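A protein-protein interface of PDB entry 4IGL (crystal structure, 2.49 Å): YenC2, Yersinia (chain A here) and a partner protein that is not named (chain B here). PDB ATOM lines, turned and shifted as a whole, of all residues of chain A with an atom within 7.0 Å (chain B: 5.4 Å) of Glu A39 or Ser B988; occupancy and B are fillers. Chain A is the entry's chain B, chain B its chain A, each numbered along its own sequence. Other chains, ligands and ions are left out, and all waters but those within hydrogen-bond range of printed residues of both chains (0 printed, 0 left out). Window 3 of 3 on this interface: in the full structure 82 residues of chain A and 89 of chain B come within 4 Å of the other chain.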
ATOM      1  N   VAL A  14     -15.089  -7.191 -26.052  1.00  0.00           N
ATOM      2  CA  VAL A  14     -14.475  -6.325 -25.048  1.00  0.00           C
ATOM      3  C   VAL A  14     -14.556  -4.874 -25.498  1.00  0.00           C
ATOM      4  O   VAL A  14     -14.153  -4.534 -26.625  1.00  0.00           O
ATOM      5  CB  VAL A  14     -12.990  -6.707 -24.781  1.00  0.00           C
ATOM      6  CG1 VAL A  14     -12.339  -5.751 -23.793  1.00  0.00           C
ATOM      7  CG2 VAL A  14     -12.879  -8.135 -24.287  1.00  0.00           C
ATOM      8  N   ARG A  23     -12.120  -5.447 -28.625  1.00  0.00           N
ATOM      9  CA  ARG A  23     -11.636  -6.830 -28.757  1.00  0.00           C
ATOM     10  C   ARG A  23     -12.712  -7.877 -29.066  1.00  0.00           C
ATOM     11  O   ARG A  23     -13.780  -7.876 -28.471  1.00  0.00           O
ATOM     12  CB  ARG A  23     -10.864  -7.260 -27.504  1.00  0.00           C
ATOM     13  CG  ARG A  23      -9.550  -6.537 -27.294  1.00  0.00           C
ATOM     14  CD  ARG A  23      -8.804  -7.056 -26.078  1.00  0.00           C
ATOM     15  NE  ARG A  23      -7.515  -6.383 -25.920  1.00  0.00           N
ATOM     16  CZ  ARG A  23      -6.503  -6.855 -25.199  1.00  0.00           C
ATOM     17  NH1 ARG A  23      -6.622  -8.017 -24.571  1.00  0.00           N
ATOM     18  NH2 ARG A  23      -5.368  -6.173 -25.123  1.00  0.00           N
ATOM     19  N   ILE A  25     -12.915 -11.843 -28.734  1.00  0.00           N
ATOM     20  CA  ILE A  25     -12.166 -12.972 -28.183  1.00  0.00           C
ATOM     21  C   ILE A  25     -12.881 -14.309 -28.396  1.00  0.00           C
ATOM     22  O   ILE A  25     -14.017 -14.504 -27.955  1.00  0.00           O
ATOM     23  CB  ILE A  25     -11.868 -12.789 -26.671  1.00  0.00           C
ATOM     24  CG1 ILE A  25     -11.215 -11.429 -26.405  1.00  0.00           C
ATOM     25  CG2 ILE A  25     -10.992 -13.930 -26.152  1.00  0.00           C
ATOM     26  CD1 ILE A  25     -10.970 -11.149 -24.930  1.00  0.00           C
ATOM     27  N   ALA A  26     -12.193 -15.223 -29.071  1.00  0.00           N
ATOM     28  CA  ALA A  26     -12.677 -16.582 -29.274  1.00  0.00           C
ATOM     29  C   ALA A  26     -11.755 -17.553 -28.558  1.00  0.00           C
ATOM     30  O   ALA A  26     -10.665 -17.183 -28.127  1.00  0.00           O
ATOM     31  CB  ALA A  26     -12.752 -16.916 -30.757  1.00  0.00           C
ATOM     32  N   TYR A  27     -12.210 -18.788 -28.410  1.00  0.00           N
ATOM     33  CA  TYR A  27     -11.439 -19.817 -27.731  1.00  0.00           C
ATOM     34  C   TYR A  27     -11.407 -21.094 -28.563  1.00  0.00           C
ATOM     35  O   TYR A  27     -12.404 -21.811 -28.653  1.00  0.00           O
ATOM     36  CB  TYR A  27     -12.012 -20.072 -26.337  1.00  0.00           C
ATOM     37  CG  TYR A  27     -11.883 -18.870 -25.427  1.00  0.00           C
ATOM     38  CD1 TYR A  27     -12.879 -17.903 -25.371  1.00  0.00           C
ATOM     39  CD2 TYR A  27     -10.755 -18.695 -24.635  1.00  0.00           C
ATOM     40  CE1 TYR A  27     -12.759 -16.797 -24.544  1.00  0.00           C
ATOM     41  CE2 TYR A  27     -10.625 -17.598 -23.804  1.00  0.00           C
ATOM     42  CZ  TYR A  27     -11.627 -16.652 -23.761  1.00  0.00           C
ATOM     43  OH  TYR A  27     -11.501 -15.558 -22.935  1.00  0.00           O
ATOM     44  N   ARG A  28     -10.262 -21.356 -29.192  1.00  0.00           N
ATOM     45  CA  ARG A  28     -10.127 -22.486 -30.104  1.00  0.00           C
ATOM     46  C   ARG A  28      -9.641 -23.747 -29.397  1.00  0.00           C
ATOM     47  O   ARG A  28      -8.603 -23.746 -28.735  1.00  0.00           O
ATOM     48  CB  ARG A  28      -9.204 -22.133 -31.274  1.00  0.00           C
ATOM     49  CG  ARG A  28      -9.070 -23.237 -32.315  1.00  0.00           C
ATOM     50  CD  ARG A  28      -8.543 -22.682 -33.633  1.00  0.00           C
ATOM     51  NE  ARG A  28      -7.154 -22.231 -33.551  1.00  0.00           N
ATOM     52  CZ  ARG A  28      -6.218 -22.498 -34.460  1.00  0.00           C
ATOM     53  NH1 ARG A  28      -6.514 -23.210 -35.539  1.00  0.00           N
ATOM     54  NH2 ARG A  28      -4.983 -22.037 -34.296  1.00  0.00           N
ATOM     55  N   THR A  37      -6.392 -24.997 -25.022  1.00  0.00           N
ATOM     56  CA  THR A  37      -7.347 -23.995 -25.473  1.00  0.00           C
ATOM     57  C   THR A  37      -6.600 -22.748 -25.924  1.00  0.00           C
ATOM     58  O   THR A  37      -5.943 -22.091 -25.120  1.00  0.00           O
ATOM     59  CB  THR A  37      -8.340 -23.611 -24.361  1.00  0.00           C
ATOM     60  OG1 THR A  37      -8.835 -24.792 -23.715  1.00  0.00           O
ATOM     61  CG2 THR A  37      -9.499 -22.802 -24.939  1.00  0.00           C
ATOM     62  N   GLU A  38      -6.710 -22.413 -27.205  1.00  0.00           N
ATOM     63  CA  GLU A  38      -6.055 -21.221 -27.723  1.00  0.00           C
ATOM     64  C   GLU A  38      -6.995 -20.030 -27.610  1.00  0.00           C
ATOM     65  O   GLU A  38      -8.126 -20.074 -28.095  1.00  0.00           O
ATOM     66  CB  GLU A  38      -5.618 -21.409 -29.179  1.00  0.00           C
ATOM     67  CG  GLU A  38      -4.870 -20.208 -29.750  1.00  0.00           C
ATOM     68  CD  GLU A  38      -4.754 -20.248 -31.264  1.00  0.00           C
ATOM     69  OE1 GLU A  38      -5.213 -21.236 -31.879  1.00  0.00           O
ATOM     70  OE2 GLU A  38      -4.219 -19.277 -31.843  1.00  0.00           O
ATOM     71  N   GLU A  39      -6.534 -18.973 -26.952  1.00  0.00           N
ATOM     72  CA  GLU A  39      -7.309 -17.744 -26.889  1.00  0.00           C
ATOM     73  C   GLU A  39      -7.001 -16.904 -28.122  1.00  0.00           C
ATOM     74  O   GLU A  39      -5.931 -16.315 -28.231  1.00  0.00           O
ATOM     75  CB  GLU A  39      -6.995 -16.973 -25.602  1.00  0.00           C
ATOM     76  CG  GLU A  39      -7.915 -15.784 -25.345  1.00  0.00           C
ATOM     77  CD  GLU A  39      -7.619 -15.074 -24.029  1.00  0.00           C
ATOM     78  OE1 GLU A  39      -6.545 -14.443 -23.917  1.00  0.00           O
ATOM     79  OE2 GLU A  39      -8.473 -15.142 -23.112  1.00  0.00           O
ATOM     80  N   CYS A  40      -7.948 -16.856 -29.053  1.00  0.00           N
ATOM     81  CA  CYS A  40      -7.768 -16.088 -30.280  1.00  0.00           C
ATOM     82  C   CYS A  40      -8.337 -14.685 -30.123  1.00  0.00           C
ATOM     83  O   CYS A  40      -9.543 -14.509 -29.967  1.00  0.00           O
ATOM     84  CB  CYS A  40      -8.449 -16.795 -31.456  1.00  0.00           C
ATOM     85  SG  CYS A  40      -7.778 -18.420 -31.871  1.00  0.00           S
ATOM     86  N   ILE A  41      -7.471 -13.680 -30.179  1.00  0.00           N
ATOM     87  CA  ILE A  41      -7.924 -12.306 -29.990  1.00  0.00           C
ATOM     88  C   ILE A  41      -7.776 -11.410 -31.227  1.00  0.00           C
ATOM     89  O   ILE A  41      -6.683 -11.222 -31.755  1.00  0.00           O
ATOM     90  CB  ILE A  41      -7.232 -11.646 -28.770  1.00  0.00           C
ATOM     91  CG1 ILE A  41      -7.452 -12.498 -27.514  1.00  0.00           C
ATOM     92  CG2 ILE A  41      -7.760 -10.234 -28.551  1.00  0.00           C
ATOM     93  CD1 ILE A  41      -6.911 -11.872 -26.239  1.00  0.00           C
ATOM     94  N   TYR A  43      -8.188  -7.591 -32.606  1.00  0.00           N
ATOM     95  CA  TYR A  43      -8.069  -6.268 -32.008  1.00  0.00           C
ATOM     96  C   TYR A  43      -8.675  -5.187 -32.893  1.00  0.00           C
ATOM     97  O   TYR A  43      -8.521  -5.206 -34.115  1.00  0.00           O
ATOM     98  CB  TYR A  43      -6.597  -5.953 -31.726  1.00  0.00           C
ATOM     99  CG  TYR A  43      -5.953  -6.899 -30.736  1.00  0.00           C
ATOM    100  CD1 TYR A  43      -5.378  -8.095 -31.157  1.00  0.00           C
ATOM    101  CD2 TYR A  43      -5.910  -6.588 -29.384  1.00  0.00           C
ATOM    102  CE1 TYR A  43      -4.788  -8.961 -30.251  1.00  0.00           C
ATOM    103  CE2 TYR A  43      -5.325  -7.444 -28.472  1.00  0.00           C
ATOM    104  CZ  TYR A  43      -4.764  -8.628 -28.909  1.00  0.00           C
ATOM    105  OH  TYR A  43      -4.184  -9.475 -27.995  1.00  0.00           O
ATOM    106  N   PRO A  58      -5.649 -12.418 -34.796  1.00  0.00           N
ATOM    107  CA  PRO A  58      -4.767 -12.957 -33.749  1.00  0.00           C
ATOM    108  C   PRO A  58      -3.372 -13.329 -34.245  1.00  0.00           C
ATOM    109  O   PRO A  58      -2.403 -13.199 -33.493  1.00  0.00           O
ATOM    110  CB  PRO A  58      -5.500 -14.221 -33.290  1.00  0.00           C
ATOM    111  CG  PRO A  58      -6.935 -13.956 -33.585  1.00  0.00           C
ATOM    112  CD  PRO A  58      -6.943 -13.129 -34.843  1.00  0.00           C
ATOM    113  N   SER A 417      -4.328 -19.301 -36.890  1.00  0.00           N
ATOM    114  CA  SER A 417      -5.056 -18.402 -35.995  1.00  0.00           C
ATOM    115  C   SER A 417      -5.987 -17.441 -36.729  1.00  0.00           C
ATOM    116  O   SER A 417      -6.935 -16.923 -36.140  1.00  0.00           O
ATOM    117  CB  SER A 417      -4.084 -17.607 -35.122  1.00  0.00           C
ATOM    118  OG  SER A 417      -3.316 -18.470 -34.305  1.00  0.00           O
ATOM    119  N   THR B 984      -8.169 -16.897 -18.396  1.00  0.00           N
ATOM    120  CA  THR B 984      -7.394 -15.812 -19.008  1.00  0.00           C
ATOM    121  C   THR B 984      -8.219 -14.571 -19.343  1.00  0.00           C
ATOM    122  O   THR B 984      -7.659 -13.503 -19.617  1.00  0.00           O
ATOM    123  CB  THR B 984      -6.701 -16.281 -20.304  1.00  0.00           C
ATOM    124  OG1 THR B 984      -7.683 -16.848 -21.183  1.00  0.00           O
ATOM    125  CG2 THR B 984      -5.638 -17.330 -20.000  1.00  0.00           C
ATOM    126  N   LEU B 985      -9.545 -14.715 -19.312  1.00  0.00           N
ATOM    127  CA  LEU B 985     -10.456 -13.664 -19.770  1.00  0.00           C
ATOM    128  C   LEU B 985     -10.302 -12.368 -18.979  1.00  0.00           C
ATOM    129  O   LEU B 985     -10.308 -11.276 -19.553  1.00  0.00           O
ATOM    130  CB  LEU B 985     -11.907 -14.154 -19.703  1.00  0.00           C
ATOM    131  CG  LEU B 985     -13.022 -13.240 -20.225  1.00  0.00           C
ATOM    132  CD1 LEU B 985     -12.758 -12.815 -21.656  1.00  0.00           C
ATOM    133  CD2 LEU B 985     -14.380 -13.926 -20.105  1.00  0.00           C
ATOM    134  N   PHE B 986     -10.146 -12.502 -17.665  1.00  0.00           N
ATOM    135  CA  PHE B 986      -9.949 -11.360 -16.773  1.00  0.00           C
ATOM    136  C   PHE B 986      -8.793 -10.468 -17.227  1.00  0.00           C
ATOM    137  O   PHE B 986      -8.962  -9.258 -17.394  1.00  0.00           O
ATOM    138  CB  PHE B 986      -9.757 -11.847 -15.325  1.00  0.00           C
ATOM    139  CG  PHE B 986      -9.322 -10.769 -14.362  1.00  0.00           C
ATOM    140  CD1 PHE B 986     -10.020  -9.572 -14.264  1.00  0.00           C
ATOM    141  CD2 PHE B 986      -8.228 -10.975 -13.528  1.00  0.00           C
ATOM    142  CE1 PHE B 986      -9.618  -8.586 -13.373  1.00  0.00           C
ATOM    143  CE2 PHE B 986      -7.821  -9.999 -12.628  1.00  0.00           C
ATOM    144  CZ  PHE B 986      -8.515  -8.804 -12.548  1.00  0.00           C
ATOM    145  N   ASP B 987      -7.629 -11.077 -17.437  1.00  0.00           N
ATOM    146  CA  ASP B 987      -6.452 -10.346 -17.892  1.00  0.00           C
ATOM    147  C   ASP B 987      -6.666  -9.811 -19.302  1.00  0.00           C
ATOM    148  O   ASP B 987      -6.320  -8.673 -19.608  1.00  0.00           O
ATOM    149  CB  ASP B 987      -5.212 -11.249 -17.885  1.00  0.00           C
ATOM    150  CG  ASP B 987      -4.880 -11.790 -16.504  1.00  0.00           C
ATOM    151  OD1 ASP B 987      -5.200 -11.127 -15.494  1.00  0.00           O
ATOM    152  OD2 ASP B 987      -4.300 -12.895 -16.435  1.00  0.00           O
ATOM    153  N   SER B 988      -7.251 -10.638 -20.161  1.00  0.00           N
ATOM    154  CA  SER B 988      -7.412 -10.281 -21.563  1.00  0.00           C
ATOM    155  C   SER B 988      -8.555  -9.289 -21.807  1.00  0.00           C
ATOM    156  O   SER B 988      -8.717  -8.786 -22.918  1.00  0.00           O
ATOM    157  CB  SER B 988      -7.593 -11.540 -22.413  1.00  0.00           C
ATOM    158  OG  SER B 988      -6.464 -12.392 -22.299  1.00  0.00           O
ATOM    159  N   SER B 989      -9.334  -9.000 -20.769  1.00  0.00           N
ATOM    160  CA  SER B 989     -10.428  -8.042 -20.897  1.00  0.00           C
ATOM    161  C   SER B 989      -9.907  -6.615 -20.776  1.00  0.00           C
ATOM    162  O   SER B 989     -10.637  -5.655 -21.018  1.00  0.00           O
ATOM    163  CB  SER B 989     -11.501  -8.279 -19.837  1.00  0.00           C
ATOM    164  OG  SER B 989     -11.050  -7.870 -18.557  1.00  0.00           O
ATOM    165  N   TYR B 990      -8.646  -6.474 -20.383  1.00  0.00           N
ATOM    166  CA  TYR B 990      -8.052  -5.146 -20.257  1.00  0.00           C
ATOM    167  C   TYR B 990      -7.389  -4.700 -21.560  1.00  0.00           C
ATOM    168  O   TYR B 990      -6.634  -5.447 -22.181  1.00  0.00           O
ATOM    169  CB  TYR B 990      -7.080  -5.083 -19.071  1.00  0.00           C
ATOM    170  CG  TYR B 990      -7.781  -5.030 -17.726  1.00  0.00           C
ATOM    171  CD1 TYR B 990      -8.291  -6.179 -17.133  1.00  0.00           C
ATOM    172  CD2 TYR B 990      -7.958  -3.820 -17.067  1.00  0.00           C
ATOM    173  CE1 TYR B 990      -8.941  -6.124 -15.907  1.00  0.00           C
ATOM    174  CE2 TYR B 990      -8.604  -3.753 -15.846  1.00  0.00           C
ATOM    175  CZ  TYR B 990      -9.095  -4.906 -15.271  1.00  0.00           C
ATOM    176  OH  TYR B 990      -9.740  -4.843 -14.059  1.00  0.00           O
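OG1 of Thr B984 is in hydrogen-bond range of OE2 of Glu A39 (2.7 Å). The backbone carbonyl oxygen of Ser B988 is in hydrogen-bond range of the guanidinium group of Arg A23, at 2.8 Å. The side-chain hydroxyl (OG) of Ser B988 lies within hydrogen-bond range of the side-chain carboxylate (OE1) of Glu A39, at 2.6 Å. O of Tyr B990 lies within hydrogen-bond range of NH2 of Arg A23.
OG of Ser B988 is in hydrogen-bond range of O of Thr B984. The backbone carbonyl oxygen of Phe B986 is in hydrogen-bond range of the side-chain hydroxyl of Ser B989, at 2.8 Å. The backbone carbonyl oxygen of Arg A23 is in hydrogen-bond range of the backbone NH of Val A14, 2.8 Å away. The side-chain hydroxyl of Tyr A27 is in hydrogen-bond range of the side-chain carboxylate of Glu A39 (3.1 Å).
CG1 of Val A14 touches O of Ser B989 (3.3 Å). Ile A25 touches Ser B988 (CD1 to O, 3.8 Å). Leu B985 touches Tyr A27. Glu A39 touches Leu B985 (OE2 to N, 3.97 Å). Ile A41 touches Ser B988 (CD1 to CB, 3.9 Å).
Printed residues of chain B within 4 Å of Val A14: Ser B989. Of the printed residues of chain B, Arg A23 touches Ser B988 (2.8 Å) and Tyr B990 (3.3 Å). Glu A39 touches three residues of chain B. Of the printed residues of chain A, Thr B984 touches Glu A39 (2.7 Å). The nearest printed residue of chain B that does not touch Glu A39 is Phe B986 (6.3 Å). The nearest printed residue of chain B that does not touch Ile A25 is Leu B985 (4.1 Å).
Hydrophobic or aromatic side chains of chain B within 4 Å of the printed part of chain A: Leu B985. Along chain A the printed residues that touch a printed residue of chain B span positions 14 to 41. Among the printed residues, 9 pairs touch across the chains. Among the printed residues, no Asp or Glu carboxylate lies within 4 Å of a Lys or Arg side-chain nitrogen of the other chain.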
